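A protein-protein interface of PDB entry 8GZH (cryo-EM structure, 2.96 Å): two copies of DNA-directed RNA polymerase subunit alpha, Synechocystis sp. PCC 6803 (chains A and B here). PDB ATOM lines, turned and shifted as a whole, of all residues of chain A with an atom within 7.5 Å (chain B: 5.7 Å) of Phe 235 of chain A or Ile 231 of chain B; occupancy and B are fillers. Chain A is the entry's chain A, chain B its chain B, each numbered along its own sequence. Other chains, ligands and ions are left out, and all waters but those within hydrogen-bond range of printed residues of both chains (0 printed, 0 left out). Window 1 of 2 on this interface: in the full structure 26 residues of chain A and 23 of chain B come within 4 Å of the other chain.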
ATOM      1  N   GLN A  46     -17.562   5.637  -8.773  1.00  0.00           N
ATOM      2  CA  GLN A  46     -16.131   5.603  -9.053  1.00  0.00           C
ATOM      3  C   GLN A  46     -15.344   5.034  -7.882  1.00  0.00           C
ATOM      4  O   GLN A  46     -14.273   4.448  -8.077  1.00  0.00           O
ATOM      5  CB  GLN A  46     -15.635   6.999  -9.414  1.00  0.00           C
ATOM      6  CG  GLN A  46     -15.992   7.407 -10.826  1.00  0.00           C
ATOM      7  CD  GLN A  46     -15.295   8.674 -11.261  1.00  0.00           C
ATOM      8  OE1 GLN A  46     -14.811   9.446 -10.435  1.00  0.00           O
ATOM      9  NE2 GLN A  46     -15.237   8.894 -12.567  1.00  0.00           N
ATOM     10  N   THR A  49     -15.572   1.333  -8.492  1.00  0.00           N
ATOM     11  CA  THR A  49     -14.709   0.959  -9.620  1.00  0.00           C
ATOM     12  C   THR A  49     -13.241   0.917  -9.213  1.00  0.00           C
ATOM     13  O   THR A  49     -12.549  -0.082  -9.466  1.00  0.00           O
ATOM     14  CB  THR A  49     -14.854   1.919 -10.803  1.00  0.00           C
ATOM     15  OG1 THR A  49     -14.348   3.208 -10.446  1.00  0.00           O
ATOM     16  CG2 THR A  49     -16.274   2.040 -11.263  1.00  0.00           C
ATOM     17  N   VAL A  50     -12.763   1.986  -8.563  1.00  0.00           N
ATOM     18  CA  VAL A  50     -11.369   2.069  -8.137  1.00  0.00           C
ATOM     19  C   VAL A  50     -11.056   0.995  -7.103  1.00  0.00           C
ATOM     20  O   VAL A  50     -10.021   0.318  -7.190  1.00  0.00           O
ATOM     21  CB  VAL A  50     -11.065   3.487  -7.611  1.00  0.00           C
ATOM     22  CG1 VAL A  50      -9.750   3.532  -6.857  1.00  0.00           C
ATOM     23  CG2 VAL A  50     -11.034   4.474  -8.760  1.00  0.00           C
ATOM     24  N   ALA A  53     -11.084  -2.626  -8.828  1.00  0.00           N
ATOM     25  CA  ALA A  53      -9.927  -2.792  -9.704  1.00  0.00           C
ATOM     26  C   ALA A  53      -8.639  -2.913  -8.901  1.00  0.00           C
ATOM     27  O   ALA A  53      -7.792  -3.768  -9.202  1.00  0.00           O
ATOM     28  CB  ALA A  53      -9.841  -1.626 -10.686  1.00  0.00           C
ATOM     29  N   SER A 228      -1.344   0.567  -8.943  1.00  0.00           N
ATOM     30  CA  SER A 228      -1.784   1.788  -9.607  1.00  0.00           C
ATOM     31  C   SER A 228      -1.158   1.933 -10.987  1.00  0.00           C
ATOM     32  O   SER A 228      -1.865   2.193 -11.968  1.00  0.00           O
ATOM     33  CB  SER A 228      -1.453   3.001  -8.741  1.00  0.00           C
ATOM     34  OG  SER A 228      -2.211   2.990  -7.548  1.00  0.00           O
ATOM     35  N   ASP A 229       0.159   1.743 -11.101  1.00  0.00           N
ATOM     36  CA  ASP A 229       0.715   1.908 -12.438  1.00  0.00           C
ATOM     37  C   ASP A 229       0.527   0.671 -13.314  1.00  0.00           C
ATOM     38  O   ASP A 229       0.599   0.802 -14.538  1.00  0.00           O
ATOM     39  CB  ASP A 229       2.184   2.375 -12.403  1.00  0.00           C
ATOM     40  CG  ASP A 229       3.142   1.387 -11.764  1.00  0.00           C
ATOM     41  OD1 ASP A 229       2.724   0.353 -11.236  1.00  0.00           O
ATOM     42  OD2 ASP A 229       4.359   1.667 -11.789  1.00  0.00           O
ATOM     43  N   ILE A 230       0.190  -0.494 -12.742  1.00  0.00           N
ATOM     44  CA  ILE A 230      -0.260  -1.612 -13.574  1.00  0.00           C
ATOM     45  C   ILE A 230      -1.603  -1.285 -14.229  1.00  0.00           C
ATOM     46  O   ILE A 230      -1.783  -1.481 -15.440  1.00  0.00           O
ATOM     47  CB  ILE A 230      -0.322  -2.910 -12.747  1.00  0.00           C
ATOM     48  CG1 ILE A 230       1.059  -3.550 -12.654  1.00  0.00           C
ATOM     49  CG2 ILE A 230      -1.274  -3.927 -13.360  1.00  0.00           C
ATOM     50  CD1 ILE A 230       1.143  -4.631 -11.608  1.00  0.00           C
ATOM     51  N   ILE A 231      -2.549  -0.745 -13.448  1.00  0.00           N
ATOM     52  CA  ILE A 231      -3.854  -0.367 -13.997  1.00  0.00           C
ATOM     53  C   ILE A 231      -3.715   0.779 -15.000  1.00  0.00           C
ATOM     54  O   ILE A 231      -4.361   0.780 -16.063  1.00  0.00           O
ATOM     55  CB  ILE A 231      -4.819  -0.020 -12.844  1.00  0.00           C
ATOM     56  CG1 ILE A 231      -5.157  -1.278 -12.052  1.00  0.00           C
ATOM     57  CG2 ILE A 231      -6.109   0.586 -13.353  1.00  0.00           C
ATOM     58  CD1 ILE A 231      -5.795  -1.011 -10.715  1.00  0.00           C
ATOM     59  N   ALA A 232      -2.825   1.737 -14.709  1.00  0.00           N
ATOM     60  CA  ALA A 232      -2.592   2.851 -15.624  1.00  0.00           C
ATOM     61  C   ALA A 232      -1.961   2.387 -16.933  1.00  0.00           C
ATOM     62  O   ALA A 232      -2.354   2.851 -18.008  1.00  0.00           O
ATOM     63  CB  ALA A 232      -1.716   3.904 -14.950  1.00  0.00           C
ATOM     64  N   ASN A 233      -0.998   1.459 -16.874  1.00  0.00           N
ATOM     65  CA  ASN A 233      -0.424   0.919 -18.098  1.00  0.00           C
ATOM     66  C   ASN A 233      -1.393   0.014 -18.845  1.00  0.00           C
ATOM     67  O   ASN A 233      -1.212  -0.208 -20.045  1.00  0.00           O
ATOM     68  CB  ASN A 233       0.859   0.149 -17.792  1.00  0.00           C
ATOM     69  CG  ASN A 233       2.000   1.056 -17.400  1.00  0.00           C
ATOM     70  OD1 ASN A 233       1.950   2.266 -17.611  1.00  0.00           O
ATOM     71  ND2 ASN A 233       3.042   0.472 -16.823  1.00  0.00           N
ATOM     72  N   LEU A 234      -2.401  -0.532 -18.163  1.00  0.00           N
ATOM     73  CA  LEU A 234      -3.456  -1.248 -18.873  1.00  0.00           C
ATOM     74  C   LEU A 234      -4.345  -0.287 -19.650  1.00  0.00           C
ATOM     75  O   LEU A 234      -4.725  -0.568 -20.792  1.00  0.00           O
ATOM     76  CB  LEU A 234      -4.298  -2.064 -17.894  1.00  0.00           C
ATOM     77  CG  LEU A 234      -3.896  -3.509 -17.610  1.00  0.00           C
ATOM     78  CD1 LEU A 234      -4.702  -4.043 -16.440  1.00  0.00           C
ATOM     79  CD2 LEU A 234      -4.086  -4.378 -18.837  1.00  0.00           C
ATOM     80  N   PHE A 235      -4.693   0.851 -19.048  1.00  0.00           N
ATOM     81  CA  PHE A 235      -5.729   1.704 -19.621  1.00  0.00           C
ATOM     82  C   PHE A 235      -5.211   2.850 -20.486  1.00  0.00           C
ATOM     83  O   PHE A 235      -6.017   3.477 -21.179  1.00  0.00           O
ATOM     84  CB  PHE A 235      -6.616   2.271 -18.509  1.00  0.00           C
ATOM     85  CG  PHE A 235      -7.678   1.320 -18.056  1.00  0.00           C
ATOM     86  CD1 PHE A 235      -7.522   0.591 -16.890  1.00  0.00           C
ATOM     87  CD2 PHE A 235      -8.824   1.136 -18.811  1.00  0.00           C
ATOM     88  CE1 PHE A 235      -8.498  -0.293 -16.478  1.00  0.00           C
ATOM     89  CE2 PHE A 235      -9.802   0.254 -18.406  1.00  0.00           C
ATOM     90  CZ  PHE A 235      -9.640  -0.461 -17.237  1.00  0.00           C
ATOM     91  N   ILE A 236      -3.916   3.149 -20.471  1.00  0.00           N
ATOM     92  CA  ILE A 236      -3.367   4.191 -21.349  1.00  0.00           C
ATOM     93  C   ILE A 236      -3.387   3.823 -22.839  1.00  0.00           C
ATOM     94  O   ILE A 236      -3.837   4.671 -23.631  1.00  0.00           O
ATOM     95  CB  ILE A 236      -1.966   4.629 -20.867  1.00  0.00           C
ATOM     96  CG1 ILE A 236      -2.092   5.592 -19.681  1.00  0.00           C
ATOM     97  CG2 ILE A 236      -1.123   5.242 -21.983  1.00  0.00           C
ATOM     98  CD1 ILE A 236      -0.791   5.853 -18.964  1.00  0.00           C
ATOM     99  N   PRO A 237      -2.961   2.628 -23.307  1.00  0.00           N
ATOM    100  CA  PRO A 237      -3.053   2.366 -24.758  1.00  0.00           C
ATOM    101  C   PRO A 237      -4.471   2.227 -25.288  1.00  0.00           C
ATOM    102  O   PRO A 237      -4.665   2.357 -26.500  1.00  0.00           O
ATOM    103  CB  PRO A 237      -2.270   1.059 -24.937  1.00  0.00           C
ATOM    104  CG  PRO A 237      -2.351   0.406 -23.644  1.00  0.00           C
ATOM    105  CD  PRO A 237      -2.230   1.517 -22.661  1.00  0.00           C
ATOM    106  N   LEU A 238      -5.463   1.983 -24.430  1.00  0.00           N
ATOM    107  CA  LEU A 238      -6.851   2.032 -24.879  1.00  0.00           C
ATOM    108  C   LEU A 238      -7.275   3.453 -25.218  1.00  0.00           C
ATOM    109  O   LEU A 238      -8.092   3.658 -26.120  1.00  0.00           O
ATOM    110  CB  LEU A 238      -7.772   1.453 -23.811  1.00  0.00           C
ATOM    111  CG  LEU A 238      -7.817  -0.064 -23.702  1.00  0.00           C
ATOM    112  CD1 LEU A 238      -8.787  -0.484 -22.615  1.00  0.00           C
ATOM    113  CD2 LEU A 238      -8.215  -0.643 -25.036  1.00  0.00           C
ATOM    114  N   LYS A 239      -6.739   4.439 -24.502  1.00  0.00           N
ATOM    115  CA  LYS A 239      -7.001   5.835 -24.821  1.00  0.00           C
ATOM    116  C   LYS A 239      -6.172   6.292 -26.015  1.00  0.00           C
ATOM    117  O   LYS A 239      -6.665   7.034 -26.871  1.00  0.00           O
ATOM    118  CB  LYS A 239      -6.710   6.707 -23.599  1.00  0.00           C
ATOM    119  CG  LYS A 239      -6.917   8.196 -23.811  1.00  0.00           C
ATOM    120  CD  LYS A 239      -5.772   9.003 -23.226  1.00  0.00           C
ATOM    121  CE  LYS A 239      -5.561   8.698 -21.752  1.00  0.00           C
ATOM    122  NZ  LYS A 239      -4.489   9.548 -21.165  1.00  0.00           N
ATOM    123  N   ASP A 240      -4.917   5.843 -26.089  1.00  0.00           N
ATOM    124  CA  ASP A 240      -4.021   6.294 -27.149  1.00  0.00           C
ATOM    125  C   ASP A 240      -4.390   5.672 -28.492  1.00  0.00           C
ATOM    126  O   ASP A 240      -4.689   6.382 -29.459  1.00  0.00           O
ATOM    127  CB  ASP A 240      -2.571   5.967 -26.778  1.00  0.00           C
ATOM    128  N   THR B  49     -11.518  -7.320 -15.047  1.00  0.00           N
ATOM    129  CA  THR B  49     -11.232  -6.020 -14.443  1.00  0.00           C
ATOM    130  C   THR B  49     -11.448  -4.887 -15.438  1.00  0.00           C
ATOM    131  O   THR B  49     -12.180  -3.925 -15.155  1.00  0.00           O
ATOM    132  CB  THR B  49      -9.792  -6.000 -13.930  1.00  0.00           C
ATOM    133  OG1 THR B  49      -9.516  -7.214 -13.224  1.00  0.00           O
ATOM    134  CG2 THR B  49      -9.572  -4.822 -13.007  1.00  0.00           C
ATOM    135  N   VAL B  50     -10.835  -5.005 -16.621  1.00  0.00           N
ATOM    136  CA  VAL B  50     -10.942  -3.973 -17.647  1.00  0.00           C
ATOM    137  C   VAL B  50     -12.377  -3.863 -18.154  1.00  0.00           C
ATOM    138  O   VAL B  50     -12.898  -2.754 -18.322  1.00  0.00           O
ATOM    139  CB  VAL B  50      -9.944  -4.258 -18.786  1.00  0.00           C
ATOM    140  CG1 VAL B  50     -10.117  -3.282 -19.931  1.00  0.00           C
ATOM    141  CG2 VAL B  50      -8.524  -4.186 -18.269  1.00  0.00           C
ATOM    142  N   ALA B  53     -14.698  -2.285 -15.263  1.00  0.00           N
ATOM    143  CA  ALA B  53     -14.392  -0.870 -15.078  1.00  0.00           C
ATOM    144  C   ALA B  53     -14.836  -0.041 -16.279  1.00  0.00           C
ATOM    145  O   ALA B  53     -15.416   1.042 -16.109  1.00  0.00           O
ATOM    146  CB  ALA B  53     -12.899  -0.685 -14.820  1.00  0.00           C
ATOM    147  N   LEU B  54     -14.616  -0.556 -17.495  1.00  0.00           N
ATOM    148  CA  LEU B  54     -15.039   0.150 -18.696  1.00  0.00           C
ATOM    149  C   LEU B  54     -16.553   0.230 -18.790  1.00  0.00           C
ATOM    150  O   LEU B  54     -17.088   1.268 -19.183  1.00  0.00           O
ATOM    151  CB  LEU B  54     -14.471  -0.531 -19.938  1.00  0.00           C
ATOM    152  CG  LEU B  54     -13.073  -0.109 -20.380  1.00  0.00           C
ATOM    153  CD1 LEU B  54     -12.613  -0.982 -21.530  1.00  0.00           C
ATOM    154  CD2 LEU B  54     -13.052   1.353 -20.768  1.00  0.00           C
ATOM    155  N   VAL B  57     -17.777   2.893 -16.089  1.00  0.00           N
ATOM    156  CA  VAL B  57     -17.469   4.274 -16.455  1.00  0.00           C
ATOM    157  C   VAL B  57     -18.228   4.682 -17.718  1.00  0.00           C
ATOM    158  O   VAL B  57     -18.693   5.823 -17.835  1.00  0.00           O
ATOM    159  CB  VAL B  57     -15.944   4.453 -16.592  1.00  0.00           C
ATOM    160  CG1 VAL B  57     -15.580   5.849 -17.076  1.00  0.00           C
ATOM    161  CG2 VAL B  57     -15.286   4.213 -15.255  1.00  0.00           C
ATOM    162  N   GLU B 226     -12.812   8.042 -24.156  1.00  0.00           N
ATOM    163  CA  GLU B 226     -13.220   8.928 -23.067  1.00  0.00           C
ATOM    164  C   GLU B 226     -13.216   8.199 -21.729  1.00  0.00           C
ATOM    165  O   GLU B 226     -12.696   8.713 -20.729  1.00  0.00           O
ATOM    166  CB  GLU B 226     -14.609   9.501 -23.354  1.00  0.00           C
ATOM    167  CG  GLU B 226     -14.694  10.392 -24.579  1.00  0.00           C
ATOM    168  CD  GLU B 226     -13.959  11.704 -24.408  1.00  0.00           C
ATOM    169  OE1 GLU B 226     -13.904  12.213 -23.268  1.00  0.00           O
ATOM    170  OE2 GLU B 226     -13.440  12.231 -25.415  1.00  0.00           O
ATOM    171  N   ALA B 227     -13.783   6.991 -21.697  1.00  0.00           N
ATOM    172  CA  ALA B 227     -13.804   6.201 -20.470  1.00  0.00           C
ATOM    173  C   ALA B 227     -12.404   5.755 -20.071  1.00  0.00           C
ATOM    174  O   ALA B 227     -12.072   5.733 -18.878  1.00  0.00           O
ATOM    175  CB  ALA B 227     -14.722   4.992 -20.643  1.00  0.00           C
ATOM    176  N   SER B 228     -11.561   5.420 -21.054  1.00  0.00           N
ATOM    177  CA  SER B 228     -10.180   5.058 -20.752  1.00  0.00           C
ATOM    178  C   SER B 228      -9.395   6.250 -20.214  1.00  0.00           C
ATOM    179  O   SER B 228      -8.560   6.090 -19.318  1.00  0.00           O
ATOM    180  CB  SER B 228      -9.509   4.485 -21.996  1.00  0.00           C
ATOM    181  OG  SER B 228     -10.136   3.278 -22.381  1.00  0.00           O
ATOM    182  N   ASP B 229      -9.676   7.451 -20.729  1.00  0.00           N
ATOM    183  CA  ASP B 229      -9.055   8.665 -20.212  1.00  0.00           C
ATOM    184  C   ASP B 229      -9.496   8.938 -18.780  1.00  0.00           C
ATOM    185  O   ASP B 229      -8.679   9.339 -17.943  1.00  0.00           O
ATOM    186  CB  ASP B 229      -9.407   9.844 -21.124  1.00  0.00           C
ATOM    187  CG  ASP B 229      -8.630  11.110 -20.797  1.00  0.00           C
ATOM    188  OD1 ASP B 229      -7.646  11.057 -20.028  1.00  0.00           O
ATOM    189  OD2 ASP B 229      -9.013  12.176 -21.321  1.00  0.00           O
ATOM    190  N   ILE B 230     -10.777   8.697 -18.478  1.00  0.00           N
ATOM    191  CA  ILE B 230     -11.288   8.891 -17.119  1.00  0.00           C
ATOM    192  C   ILE B 230     -10.623   7.922 -16.143  1.00  0.00           C
ATOM    193  O   ILE B 230     -10.181   8.322 -15.057  1.00  0.00           O
ATOM    194  CB  ILE B 230     -12.823   8.757 -17.108  1.00  0.00           C
ATOM    195  CG1 ILE B 230     -13.467   9.969 -17.776  1.00  0.00           C
ATOM    196  CG2 ILE B 230     -13.358   8.615 -15.691  1.00  0.00           C
ATOM    197  CD1 ILE B 230     -14.947   9.825 -18.005  1.00  0.00           C
ATOM    198  N   ILE B 231     -10.486   6.651 -16.535  1.00  0.00           N
ATOM    199  CA  ILE B 231      -9.882   5.657 -15.646  1.00  0.00           C
ATOM    200  C   ILE B 231      -8.384   5.918 -15.467  1.00  0.00           C
ATOM    201  O   ILE B 231      -7.845   5.792 -14.355  1.00  0.00           O
ATOM    202  CB  ILE B 231     -10.167   4.237 -16.169  1.00  0.00           C
ATOM    203  CG1 ILE B 231     -11.668   3.969 -16.173  1.00  0.00           C
ATOM    204  CG2 ILE B 231      -9.505   3.185 -15.302  1.00  0.00           C
ATOM    205  CD1 ILE B 231     -12.063   2.735 -16.934  1.00  0.00           C
ATOM    206  N   ALA B 232      -7.698   6.326 -16.541  1.00  0.00           N
ATOM    207  CA  ALA B 232      -6.273   6.626 -16.440  1.00  0.00           C
ATOM    208  C   ALA B 232      -6.020   7.861 -15.585  1.00  0.00           C
ATOM    209  O   ALA B 232      -5.076   7.881 -14.790  1.00  0.00           O
ATOM    210  CB  ALA B 232      -5.674   6.806 -17.833  1.00  0.00           C
ATOM    211  N   ASN B 233      -6.860   8.892 -15.708  1.00  0.00           N
ATOM    212  CA  ASN B 233      -6.726  10.050 -14.832  1.00  0.00           C
ATOM    213  C   ASN B 233      -7.146   9.743 -13.401  1.00  0.00           C
ATOM    214  O   ASN B 233      -6.738  10.462 -12.485  1.00  0.00           O
ATOM    215  CB  ASN B 233      -7.544  11.223 -15.370  1.00  0.00           C
ATOM    216  CG  ASN B 233      -7.023  11.734 -16.693  1.00  0.00           C
ATOM    217  OD1 ASN B 233      -5.829  11.665 -16.970  1.00  0.00           O
ATOM    218  ND2 ASN B 233      -7.922  12.249 -17.522  1.00  0.00           N
ATOM    219  N   LEU B 234      -7.960   8.708 -13.192  1.00  0.00           N
ATOM    220  CA  LEU B 234      -8.263   8.282 -11.831  1.00  0.00           C
ATOM    221  C   LEU B 234      -7.075   7.575 -11.194  1.00  0.00           C
ATOM    222  O   LEU B 234      -6.810   7.752 -10.000  1.00  0.00           O
ATOM    223  CB  LEU B 234      -9.482   7.364 -11.823  1.00  0.00           C
ATOM    224  CG  LEU B 234     -10.857   8.019 -11.736  1.00  0.00           C
ATOM    225  CD1 LEU B 234     -11.940   6.963 -11.844  1.00  0.00           C
ATOM    226  CD2 LEU B 234     -10.983   8.790 -10.441  1.00  0.00           C
ATOM    227  N   PHE B 235      -6.350   6.768 -11.967  1.00  0.00           N
ATOM    228  CA  PHE B 235      -5.336   5.900 -11.380  1.00  0.00           C
ATOM    229  C   PHE B 235      -3.906   6.423 -11.492  1.00  0.00           C
ATOM    230  O   PHE B 235      -3.020   5.869 -10.835  1.00  0.00           O
ATOM    231  CB  PHE B 235      -5.412   4.504 -12.004  1.00  0.00           C
ATOM    232  CG  PHE B 235      -6.470   3.638 -11.396  1.00  0.00           C
ATOM    233  CD1 PHE B 235      -6.223   2.942 -10.225  1.00  0.00           C
ATOM    234  CD2 PHE B 235      -7.719   3.538 -11.982  1.00  0.00           C
ATOM    235  CE1 PHE B 235      -7.197   2.153  -9.659  1.00  0.00           C
ATOM    236  CE2 PHE B 235      -8.695   2.747 -11.424  1.00  0.00           C
ATOM    237  CZ  PHE B 235      -8.433   2.052 -10.262  1.00  0.00           C
ATOM    238  N   ILE B 236      -3.652   7.456 -12.289  1.00  0.00           N
ATOM    239  CA  ILE B 236      -2.298   8.010 -12.418  1.00  0.00           C
ATOM    240  C   ILE B 236      -1.810   8.758 -11.167  1.00  0.00           C
ATOM    241  O   ILE B 236      -0.666   8.503 -10.761  1.00  0.00           O
ATOM    242  CB  ILE B 236      -2.186   8.860 -13.705  1.00  0.00           C
ATOM    243  CG1 ILE B 236      -1.841   7.964 -14.897  1.00  0.00           C
ATOM    244  CG2 ILE B 236      -1.150   9.977 -13.593  1.00  0.00           C
ATOM    245  CD1 ILE B 236      -2.007   8.639 -16.238  1.00  0.00           C
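NZ of Lys 239 of chain A is in salt-bridge range of OD1 of Asp 229 of chain B (3.7 Å).
The backbone carbonyl oxygen (O) of Gln 46 of chain A sits at hydrogen-bond distance from the side-chain hydroxyl (OG1) of Thr 49 of chain A (2.7 Å).
OD1 of Asp 229 of chain B is in hydrogen-bond range of ND2 of Asn 233 of chain B (2.8 Å).
Among the printed residues, merely in contact across the chains: Leu 238 of chain A with Ser 228 of chain B (3.3 Å), Ile 231 of chain A with Phe 235 of chain B (3.6 Å), Val 50 of chain A with Phe 235 of chain B (3.6 Å), Phe 235 of chain A with Ile 231 of chain B (3.6 Å), Gln 46 of chain A with Ile 230 of chain B (3.7 Å), Phe 235 of chain A with Ser 228 of chain B (3.7 Å), Lys 239 of chain A with Ser 228 of chain B (3.7 Å), Phe 235 of chain A with Val 50 of chain B (3.8 Å), Gln 46 of chain A with Leu 234 of chain B (3.8 Å), Phe 235 of chain A with Leu 54 of chain B (3.8 Å), Ser 228 of chain A with Phe 235 of chain B (3.9 Å), Ala 53 of chain A with Thr 49 of chain B (3.9 Å) and Ala 53 of chain A with Phe 235 of chain B (3.96 Å).
Phe 235 of chain A touches just these residues of chain B: Val 50 (3.8 Å), Leu 54 (3.8 Å), Ser 228 (3.7 Å) and Ile 231 (3.6 Å).
Ile 231 of chain B touches just one residue of chain A: Phe 235.
Of the printed residues of chain B, Ser 228 of chain A touches Phe 235.
Of the printed residues of chain A, Ser 228 of chain B touches Phe 235 (3.7 Å), Leu 238 (3.3 Å) and Lys 239 (3.7 Å).
Printed residues of chain B within 4 Å of Ile 231 of chain A: Phe 235 (3.6 Å).
The nearest printed residue of chain A that does not touch Phe 235 of chain B is Ala 232 of chain A (4.7 Å).
Hydrophobic or aromatic side chains of chain B that line the printed part of chain A: Val 50, Leu 54, Ile 230, Ile 231, Leu 234 and Phe 235.
Of the 17 printed residues of chain A, 8 touch a printed residue of chain B.
Printed residues of chain A that touch a printed residue of chain B: Gln 46, Val 50, Ala 53, Ser 228, Ile 231, Phe 235, Leu 238 and Lys 239.
Hydrophobic or aromatic side chains of chain A that line the printed part of chain B: Val 50, Ala 53, Ile 231, Phe 235 and Leu 238.
Among the printed residues, 14 pairs touch across the chains.
Among the printed residues, Asp or Glu carboxylates within 4 Å of a Lys or Arg side-chain nitrogen of the other chain: Lys 239 of chain A with Asp 229 of chain B (3.7 Å).
Val 50 of chain A touches Phe 235 of chain B, and with the chains exchanged Phe 235 of chain A touches Val 50 of chain B.
Ala 53 of chain A touches Thr 49 of chain B, but with the chains exchanged Thr 49 of chain A does not touch Ala 53 of chain B (5.0 Å).
Ser 228 of chain A touches Phe 235 of chain B, and with the chains exchanged Phe 235 of chain A touches Ser 228 of chain B.
Ile 231 of chain A touches Phe 235 of chain B, and with the chains exchanged Phe 235 of chain A touches Ile 231 of chain B.
Of the 14 pairs that touch across the chains among the printed residues, 6 have their exchanged pair printed and touching as well.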
